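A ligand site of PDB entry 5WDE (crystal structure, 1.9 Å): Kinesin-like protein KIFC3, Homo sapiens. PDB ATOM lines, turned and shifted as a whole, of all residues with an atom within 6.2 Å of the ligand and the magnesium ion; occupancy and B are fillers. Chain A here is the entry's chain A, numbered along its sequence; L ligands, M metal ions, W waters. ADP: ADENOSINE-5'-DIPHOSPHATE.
The backbone NH (N) of Gly 93 is in hydrogen-bond range of an oxygen (O3A) of the ligand, 3.0 Å away.
The backbone NH of Ala 92 sits at hydrogen-bond distance from an oxygen (O2B) of the ligand (3.4 Å).
The backbone NH (N) of Tyr 96 is in hydrogen-bond range of an oxygen (O2A) of the ligand, at 2.7 Å.
The backbone NH of Gly 91 is in hydrogen-bond range of an oxygen (O1B) of the ligand (2.7 Å).
The side-chain amino group (NZ) of Lys 94 lies within salt-bridge range of an oxygen (O2B) of the ligand.
The backbone NH (N) of Lys 94 lies within hydrogen-bond range of an oxygen (O2B) of the ligand (2.9 Å).
The backbone NH (N) of Thr 95 is in hydrogen-bond range of an oxygen (O2A) of the ligand, 3.3 Å away.
The guanidinium group (NH1) of Arg 11 is in hydrogen-bond range of the side-chain amide oxygen (OE1) of Gln 62 (2.8 Å).
The guanidinium group (NH1) of Arg 11 sits at hydrogen-bond distance from the side-chain hydroxyl (OG1) of Thr 97.
The backbone carbonyl oxygen of Ala 92 lies within hydrogen-bond range of the side-chain amide nitrogen of Gln 304, 3.0 Å away.
O of Gly 93 sits at hydrogen-bond distance from NE2 of Gln 304, 3.4 Å away.
The backbone carbonyl oxygen (O) of Ala 60 sits at hydrogen-bond distance from the guanidinium group (NH2) of Arg 11, 3.1 Å away.
The backbone carbonyl oxygen of Gly 91 sits at hydrogen-bond distance from the guanidinium group of Arg 13 (2.8 Å).
NZ of Lys 94 sits at hydrogen-bond distance from O of Gln 89 (3.1 Å).
O of Tyr 96 is in hydrogen-bond range of NE2 of Gln 62 (3.0 Å).
N6 of the ligand lies close to NH2 of Arg 11.
CB of Arg 13 touches N7 of the ligand (3.6 Å).
Pro 14 touches the ligand (CD to N1, 3.4 Å).
CG2 of Thr 16 touches O4' of the ligand, at 3.3 Å.
Gln 89 touches the ligand.
Thr 90 touches the ligand.
Hydrophobic or aromatic side chains that line the ligand: Pro 14 and Tyr 96.
Within 4 Å of the ligand: Arg 11, Arg 13, Pro 14, Thr 16, Gln 89, Thr 90, Gly 91, Ala 92, Gly 93, Lys 94, Thr 95 and Tyr 96.
Within 4 Å of the magnesium ion: Thr 95.
The nearest printed residue that does not touch the magnesium ion is Asp 234 (4.1 Å).
Water W5 binds the magnesium ion.
The magnesium ion is bound by water W4, 2.1 Å away.
The magnesium ion is bound by OG1 of Thr 95.
O3B of the ligand is bound to the magnesium ion.
Water W1 binds the magnesium ion (2.2 Å).
Water W2 is bound to the magnesium ion (2.2 Å).
The magnesium ion has six donor atoms within binding distance.
Water W6 lies within hydrogen-bond range of a nitrogen (N7) of the ligand (2.7 Å), the side-chain hydroxyl (OG1) of Thr 97 (3.0 Å), the side-chain amide nitrogen (NE2) of Gln 304 (3.0 Å) and the backbone carbonyl oxygen (O) of Gly 93 (3.2 Å).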
ATOM      1  N   ARG A  11      30.118  35.579  23.907  1.00  0.00           N
ATOM      2  CA  ARG A  11      29.767  35.350  25.304  1.00  0.00           C
ATOM      3  C   ARG A  11      30.998  34.827  26.019  1.00  0.00           C
ATOM      4  O   ARG A  11      31.568  33.809  25.622  1.00  0.00           O
ATOM      5  CB  ARG A  11      28.604  34.358  25.446  1.00  0.00           C
ATOM      6  CG  ARG A  11      28.162  34.246  26.903  1.00  0.00           C
ATOM      7  CD  ARG A  11      27.000  33.270  27.112  1.00  0.00           C
ATOM      8  NE  ARG A  11      26.461  33.421  28.462  1.00  0.00           N
ATOM      9  CZ  ARG A  11      25.438  32.708  28.935  1.00  0.00           C
ATOM     10  NH1 ARG A  11      24.871  31.794  28.159  1.00  0.00           N
ATOM     11  NH2 ARG A  11      24.987  32.923  30.167  1.00  0.00           N
ATOM     12  N   VAL A  12      31.412  35.542  27.063  1.00  0.00           N
ATOM     13  CA  VAL A  12      32.527  35.136  27.921  1.00  0.00           C
ATOM     14  C   VAL A  12      31.947  34.377  29.107  1.00  0.00           C
ATOM     15  O   VAL A  12      31.200  34.950  29.904  1.00  0.00           O
ATOM     16  CB  VAL A  12      33.328  36.354  28.415  1.00  0.00           C
ATOM     17  CG1 VAL A  12      34.558  35.906  29.180  1.00  0.00           C
ATOM     18  CG2 VAL A  12      33.698  37.266  27.247  1.00  0.00           C
ATOM     19  N   ARG A  13      32.264  33.092  29.219  1.00  0.00           N
ATOM     20  CA  ARG A  13      31.734  32.341  30.345  1.00  0.00           C
ATOM     21  C   ARG A  13      32.520  32.670  31.611  1.00  0.00           C
ATOM     22  O   ARG A  13      33.643  33.174  31.538  1.00  0.00           O
ATOM     23  CB  ARG A  13      31.799  30.837  30.059  1.00  0.00           C
ATOM     24  CG  ARG A  13      33.194  30.268  29.947  1.00  0.00           C
ATOM     25  CD  ARG A  13      33.206  28.785  30.296  1.00  0.00           C
ATOM     26  NE  ARG A  13      34.488  28.152  30.001  1.00  0.00           N
ATOM     27  CZ  ARG A  13      35.585  28.290  30.742  1.00  0.00           C
ATOM     28  NH1 ARG A  13      35.552  29.055  31.829  1.00  0.00           N
ATOM     29  NH2 ARG A  13      36.700  27.678  30.401  1.00  0.00           N
ATOM     30  N   PRO A  14      31.943  32.430  32.786  1.00  0.00           N
ATOM     31  CA  PRO A  14      32.717  32.583  34.027  1.00  0.00           C
ATOM     32  C   PRO A  14      33.752  31.482  34.157  1.00  0.00           C
ATOM     33  O   PRO A  14      33.767  30.491  33.415  1.00  0.00           O
ATOM     34  CB  PRO A  14      31.653  32.490  35.136  1.00  0.00           C
ATOM     35  CG  PRO A  14      30.462  31.856  34.493  1.00  0.00           C
ATOM     36  CD  PRO A  14      30.515  32.164  33.023  1.00  0.00           C
ATOM     37  N   THR A  16      35.546  28.262  35.394  1.00  0.00           N
ATOM     38  CA  THR A  16      35.035  26.950  35.766  1.00  0.00           C
ATOM     39  C   THR A  16      36.118  26.163  36.484  1.00  0.00           C
ATOM     40  O   THR A  16      37.289  26.563  36.529  1.00  0.00           O
ATOM     41  CB  THR A  16      34.538  26.170  34.539  1.00  0.00           C
ATOM     42  OG1 THR A  16      35.599  26.068  33.586  1.00  0.00           O
ATOM     43  CG2 THR A  16      33.358  26.877  33.893  1.00  0.00           C
ATOM     44  N   PRO A  58      30.988  37.543  31.805  1.00  0.00           N
ATOM     45  CA  PRO A  58      30.660  36.406  32.677  1.00  0.00           C
ATOM     46  C   PRO A  58      29.464  36.644  33.603  1.00  0.00           C
ATOM     47  O   PRO A  58      28.987  35.669  34.196  1.00  0.00           O
ATOM     48  CB  PRO A  58      31.945  36.191  33.482  1.00  0.00           C
ATOM     49  CG  PRO A  58      33.022  36.684  32.590  1.00  0.00           C
ATOM     50  CD  PRO A  58      32.423  37.873  31.864  1.00  0.00           C
ATOM     51  N   ALA A  60      26.540  37.826  32.413  1.00  0.00           N
ATOM     52  CA  ALA A  60      25.328  37.773  31.601  1.00  0.00           C
ATOM     53  C   ALA A  60      24.530  36.510  31.911  1.00  0.00           C
ATOM     54  O   ALA A  60      25.078  35.412  31.939  1.00  0.00           O
ATOM     55  CB  ALA A  60      25.677  37.838  30.121  1.00  0.00           C
ATOM     56  N   GLN A  62      21.178  33.766  31.284  1.00  0.00           N
ATOM     57  CA  GLN A  62      20.521  33.170  30.136  1.00  0.00           C
ATOM     58  C   GLN A  62      19.449  34.101  29.568  1.00  0.00           C
ATOM     59  O   GLN A  62      19.278  34.196  28.353  1.00  0.00           O
ATOM     60  CB  GLN A  62      19.898  31.811  30.515  1.00  0.00           C
ATOM     61  CG  GLN A  62      20.858  30.776  31.097  1.00  0.00           C
ATOM     62  CD  GLN A  62      21.778  30.126  30.043  1.00  0.00           C
ATOM     63  OE1 GLN A  62      22.530  30.822  29.357  1.00  0.00           O
ATOM     64  NE2 GLN A  62      21.710  28.808  29.918  1.00  0.00           N
ATOM     65  N   GLY A  88      32.965  27.809  19.288  1.00  0.00           N
ATOM     66  CA  GLY A  88      34.061  28.017  20.224  1.00  0.00           C
ATOM     67  C   GLY A  88      34.694  26.720  20.685  1.00  0.00           C
ATOM     68  O   GLY A  88      34.208  25.632  20.329  1.00  0.00           O
ATOM     69  N   GLN A  89      35.754  26.804  21.474  1.00  0.00           N
ATOM     70  CA  GLN A  89      36.474  25.593  21.854  1.00  0.00           C
ATOM     71  C   GLN A  89      35.633  24.761  22.814  1.00  0.00           C
ATOM     72  O   GLN A  89      34.774  25.278  23.524  1.00  0.00           O
ATOM     73  CB  GLN A  89      37.827  25.935  22.494  1.00  0.00           C
ATOM     74  CG  GLN A  89      37.712  26.479  23.916  1.00  0.00           C
ATOM     75  CD  GLN A  89      39.067  26.797  24.560  1.00  0.00           C
ATOM     76  OE1 GLN A  89      39.263  27.894  25.093  1.00  0.00           O
ATOM     77  NE2 GLN A  89      39.989  25.833  24.540  1.00  0.00           N
ATOM     78  N   THR A  90      35.877  23.445  22.815  1.00  0.00           N
ATOM     79  CA  THR A  90      35.285  22.583  23.819  1.00  0.00           C
ATOM     80  C   THR A  90      35.589  23.143  25.204  1.00  0.00           C
ATOM     81  O   THR A  90      36.731  23.486  25.513  1.00  0.00           O
ATOM     82  CB  THR A  90      35.841  21.161  23.689  1.00  0.00           C
ATOM     83  OG1 THR A  90      35.552  20.656  22.370  1.00  0.00           O
ATOM     84  CG2 THR A  90      35.203  20.225  24.705  1.00  0.00           C
ATOM     85  N   GLY A  91      34.549  23.246  26.034  1.00  0.00           N
ATOM     86  CA  GLY A  91      34.678  23.810  27.358  1.00  0.00           C
ATOM     87  C   GLY A  91      34.311  25.292  27.452  1.00  0.00           C
ATOM     88  O   GLY A  91      34.236  25.813  28.568  1.00  0.00           O
ATOM     89  N   ALA A  92      34.077  25.962  26.323  1.00  0.00           N
ATOM     90  CA  ALA A  92      33.825  27.394  26.353  1.00  0.00           C
ATOM     91  C   ALA A  92      32.369  27.754  26.638  1.00  0.00           C
ATOM     92  O   ALA A  92      32.088  28.927  26.900  1.00  0.00           O
ATOM     93  CB  ALA A  92      34.255  28.036  25.032  1.00  0.00           C
ATOM     94  N   GLY A  93      31.456  26.792  26.593  1.00  0.00           N
ATOM     95  CA  GLY A  93      30.083  27.025  26.990  1.00  0.00           C
ATOM     96  C   GLY A  93      29.026  26.998  25.895  1.00  0.00           C
ATOM     97  O   GLY A  93      27.947  27.570  26.082  1.00  0.00           O
ATOM     98  N   LYS A  94      29.309  26.349  24.757  1.00  0.00           N
ATOM     99  CA  LYS A  94      28.333  26.276  23.671  1.00  0.00           C
ATOM    100  C   LYS A  94      27.051  25.586  24.140  1.00  0.00           C
ATOM    101  O   LYS A  94      25.947  26.114  23.984  1.00  0.00           O
ATOM    102  CB  LYS A  94      28.917  25.530  22.467  1.00  0.00           C
ATOM    103  CG  LYS A  94      30.171  26.173  21.883  1.00  0.00           C
ATOM    104  CD  LYS A  94      30.652  25.383  20.657  1.00  0.00           C
ATOM    105  CE  LYS A  94      31.170  23.995  21.043  1.00  0.00           C
ATOM    106  NZ  LYS A  94      32.367  24.072  21.954  1.00  0.00           N
ATOM    107  N   THR A  95      27.197  24.386  24.728  1.00  0.00           N
ATOM    108  CA  THR A  95      26.011  23.625  25.116  1.00  0.00           C
ATOM    109  C   THR A  95      25.279  24.298  26.270  1.00  0.00           C
ATOM    110  O   THR A  95      24.039  24.311  26.301  1.00  0.00           O
ATOM    111  CB  THR A  95      26.423  22.187  25.468  1.00  0.00           C
ATOM    112  OG1 THR A  95      27.062  21.576  24.340  1.00  0.00           O
ATOM    113  CG2 THR A  95      25.196  21.340  25.865  1.00  0.00           C
ATOM    114  N   TYR A  96      26.020  24.881  27.218  1.00  0.00           N
ATOM    115  CA  TYR A  96      25.367  25.649  28.273  1.00  0.00           C
ATOM    116  C   TYR A  96      24.510  26.768  27.682  1.00  0.00           C
ATOM    117  O   TYR A  96      23.384  26.991  28.140  1.00  0.00           O
ATOM    118  CB  TYR A  96      26.400  26.241  29.225  1.00  0.00           C
ATOM    119  CG  TYR A  96      25.772  26.992  30.389  1.00  0.00           C
ATOM    120  CD1 TYR A  96      25.456  28.344  30.273  1.00  0.00           C
ATOM    121  CD2 TYR A  96      25.485  26.340  31.582  1.00  0.00           C
ATOM    122  CE1 TYR A  96      24.866  29.022  31.325  1.00  0.00           C
ATOM    123  CE2 TYR A  96      24.899  27.027  32.637  1.00  0.00           C
ATOM    124  CZ  TYR A  96      24.599  28.365  32.507  1.00  0.00           C
ATOM    125  OH  TYR A  96      24.022  29.051  33.551  1.00  0.00           O
ATOM    126  N   THR A  97      25.020  27.463  26.676  1.00  0.00           N
ATOM    127  CA  THR A  97      24.235  28.547  26.077  1.00  0.00           C
ATOM    128  C   THR A  97      23.034  28.006  25.303  1.00  0.00           C
ATOM    129  O   THR A  97      21.945  28.586  25.347  1.00  0.00           O
ATOM    130  CB  THR A  97      25.146  29.385  25.160  1.00  0.00           C
ATOM    131  OG1 THR A  97      26.007  30.187  25.980  1.00  0.00           O
ATOM    132  CG2 THR A  97      24.325  30.299  24.248  1.00  0.00           C
ATOM    133  N   THR A 101      20.728  24.257  31.659  1.00  0.00           N
ATOM    134  CA  THR A 101      20.465  23.265  32.683  1.00  0.00           C
ATOM    135  C   THR A 101      19.016  23.394  33.125  1.00  0.00           C
ATOM    136  O   THR A 101      18.306  24.313  32.710  1.00  0.00           O
ATOM    137  CB  THR A 101      21.382  23.437  33.897  1.00  0.00           C
ATOM    138  OG1 THR A 101      21.047  24.660  34.554  1.00  0.00           O
ATOM    139  CG2 THR A 101      22.846  23.495  33.472  1.00  0.00           C
ATOM    140  N   SER A 204      30.071  14.235  21.599  1.00  0.00           N
ATOM    141  CA  SER A 204      29.338  15.364  21.043  1.00  0.00           C
ATOM    142  C   SER A 204      30.259  16.537  20.688  1.00  0.00           C
ATOM    143  O   SER A 204      29.912  17.338  19.810  1.00  0.00           O
ATOM    144  CB  SER A 204      28.269  15.824  22.027  1.00  0.00           C
ATOM    145  OG  SER A 204      28.869  16.274  23.230  1.00  0.00           O
ATOM    146  N   SER A 205      31.439  16.639  21.317  1.00  0.00           N
ATOM    147  CA  SER A 205      32.358  17.730  21.024  1.00  0.00           C
ATOM    148  C   SER A 205      32.956  17.668  19.625  1.00  0.00           C
ATOM    149  O   SER A 205      33.529  18.668  19.173  1.00  0.00           O
ATOM    150  CB  SER A 205      33.503  17.755  22.046  1.00  0.00           C
ATOM    151  OG  SER A 205      34.285  16.573  21.928  1.00  0.00           O
ATOM    152  N   ASP A 234      24.598  23.648  17.618  1.00  0.00           N
ATOM    153  CA  ASP A 234      25.666  23.524  18.602  1.00  0.00           C
ATOM    154  C   ASP A 234      26.860  22.913  17.847  1.00  0.00           C
ATOM    155  O   ASP A 234      26.906  21.702  17.606  1.00  0.00           O
ATOM    156  CB  ASP A 234      25.176  22.640  19.755  1.00  0.00           C
ATOM    157  CG  ASP A 234      26.144  22.553  20.913  1.00  0.00           C
ATOM    158  OD1 ASP A 234      27.307  23.028  20.812  1.00  0.00           O
ATOM    159  OD2 ASP A 234      25.723  21.981  21.952  1.00  0.00           O
ATOM    160  N   LEU A 235      27.803  23.768  17.452  1.00  0.00           N
ATOM    161  CA  LEU A 235      28.879  23.339  16.548  1.00  0.00           C
ATOM    162  C   LEU A 235      29.905  22.454  17.262  1.00  0.00           C
ATOM    163  O   LEU A 235      30.062  22.495  18.482  1.00  0.00           O
ATOM    164  CB  LEU A 235      29.595  24.564  15.959  1.00  0.00           C
ATOM    165  CG  LEU A 235      28.713  25.453  15.061  1.00  0.00           C
ATOM    166  CD1 LEU A 235      29.354  26.848  14.856  1.00  0.00           C
ATOM    167  CD2 LEU A 235      28.472  24.759  13.723  1.00  0.00           C
ATOM    168  N   GLN A 304      31.619  31.649  21.870  1.00  0.00           N
ATOM    169  CA  GLN A 304      31.903  31.373  23.277  1.00  0.00           C
ATOM    170  C   GLN A 304      33.408  31.405  23.527  1.00  0.00           C
ATOM    171  O   GLN A 304      34.179  30.803  22.764  1.00  0.00           O
ATOM    172  CB  GLN A 304      31.367  29.988  23.671  1.00  0.00           C
ATOM    173  CG  GLN A 304      29.865  29.818  23.519  1.00  0.00           C
ATOM    174  CD  GLN A 304      29.091  30.465  24.666  1.00  0.00           C
ATOM    175  OE1 GLN A 304      27.972  30.928  24.483  1.00  0.00           O
ATOM    176  NE2 GLN A 304      29.689  30.464  25.866  1.00  0.00           N
HETATM  177  PB  ADP L   1      31.044  23.272  25.359  1.00  0.00           P
HETATM  178  O1B ADP L   1      32.103  22.217  25.450  1.00  0.00           O
HETATM  179  O2B ADP L   1      31.496  24.491  24.581  1.00  0.00           O
HETATM  180  O3B ADP L   1      29.657  22.800  24.975  1.00  0.00           O
HETATM  181  PA  ADP L   1      29.850  23.382  27.998  1.00  0.00           P
HETATM  182  O1A ADP L   1      30.035  21.906  28.236  1.00  0.00           O
HETATM  183  O2A ADP L   1      28.494  23.984  27.716  1.00  0.00           O
HETATM  184  O3A ADP L   1      30.902  23.836  26.869  1.00  0.00           O
HETATM  185  O5' ADP L   1      30.451  24.174  29.279  1.00  0.00           O
HETATM  186  C5' ADP L   1      31.628  23.745  29.967  1.00  0.00           C
HETATM  187  C4' ADP L   1      31.429  24.005  31.459  1.00  0.00           C
HETATM  188  O4' ADP L   1      31.304  25.409  31.709  1.00  0.00           O
HETATM  189  C3' ADP L   1      30.152  23.357  31.928  1.00  0.00           C
HETATM  190  O3' ADP L   1      30.386  22.742  33.185  1.00  0.00           O
HETATM  191  C2' ADP L   1      29.166  24.491  32.105  1.00  0.00           C
HETATM  192  O2' ADP L   1      28.304  24.244  33.217  1.00  0.00           O
HETATM  193  C1' ADP L   1      30.066  25.693  32.347  1.00  0.00           C
HETATM  194  N9  ADP L   1      29.530  26.940  31.729  1.00  0.00           N
HETATM  195  C8  ADP L   1      29.606  27.270  30.430  1.00  0.00           C
HETATM  196  N7  ADP L   1      29.048  28.478  30.205  1.00  0.00           N
HETATM  197  C5  ADP L   1      28.607  28.944  31.388  1.00  0.00           C
HETATM  198  C6  ADP L   1      27.927  30.171  31.859  1.00  0.00           C
HETATM  199  N6  ADP L   1      27.596  31.160  30.999  1.00  0.00           N
HETATM  200  N1  ADP L   1      27.649  30.256  33.171  1.00  0.00           N
HETATM  201  C2  ADP L   1      27.974  29.279  34.035  1.00  0.00           C
HETATM  202  N3  ADP L   1      28.604  28.150  33.682  1.00  0.00           N
HETATM  203  C4  ADP L   1      28.932  27.933  32.387  1.00  0.00           C
HETATM  204 MG    MG M   1      29.062  20.931  24.137  1.00  0.00          MG
HETATM  205  O   HOH W   1      28.270  18.984  23.682  1.00  0.00           O
HETATM  206  O   HOH W   2      31.137  20.243  23.996  1.00  0.00           O
HETATM  207  O   HOH W   3      32.549  20.751  27.592  1.00  0.00           O
HETATM  208  O   HOH W   4      28.966  20.251  26.130  1.00  0.00           O
HETATM  209  O   HOH W   5      28.985  21.530  22.206  1.00  0.00           O
HETATM  210  O   HOH W   6      27.921  29.997  28.219  1.00  0.00           O
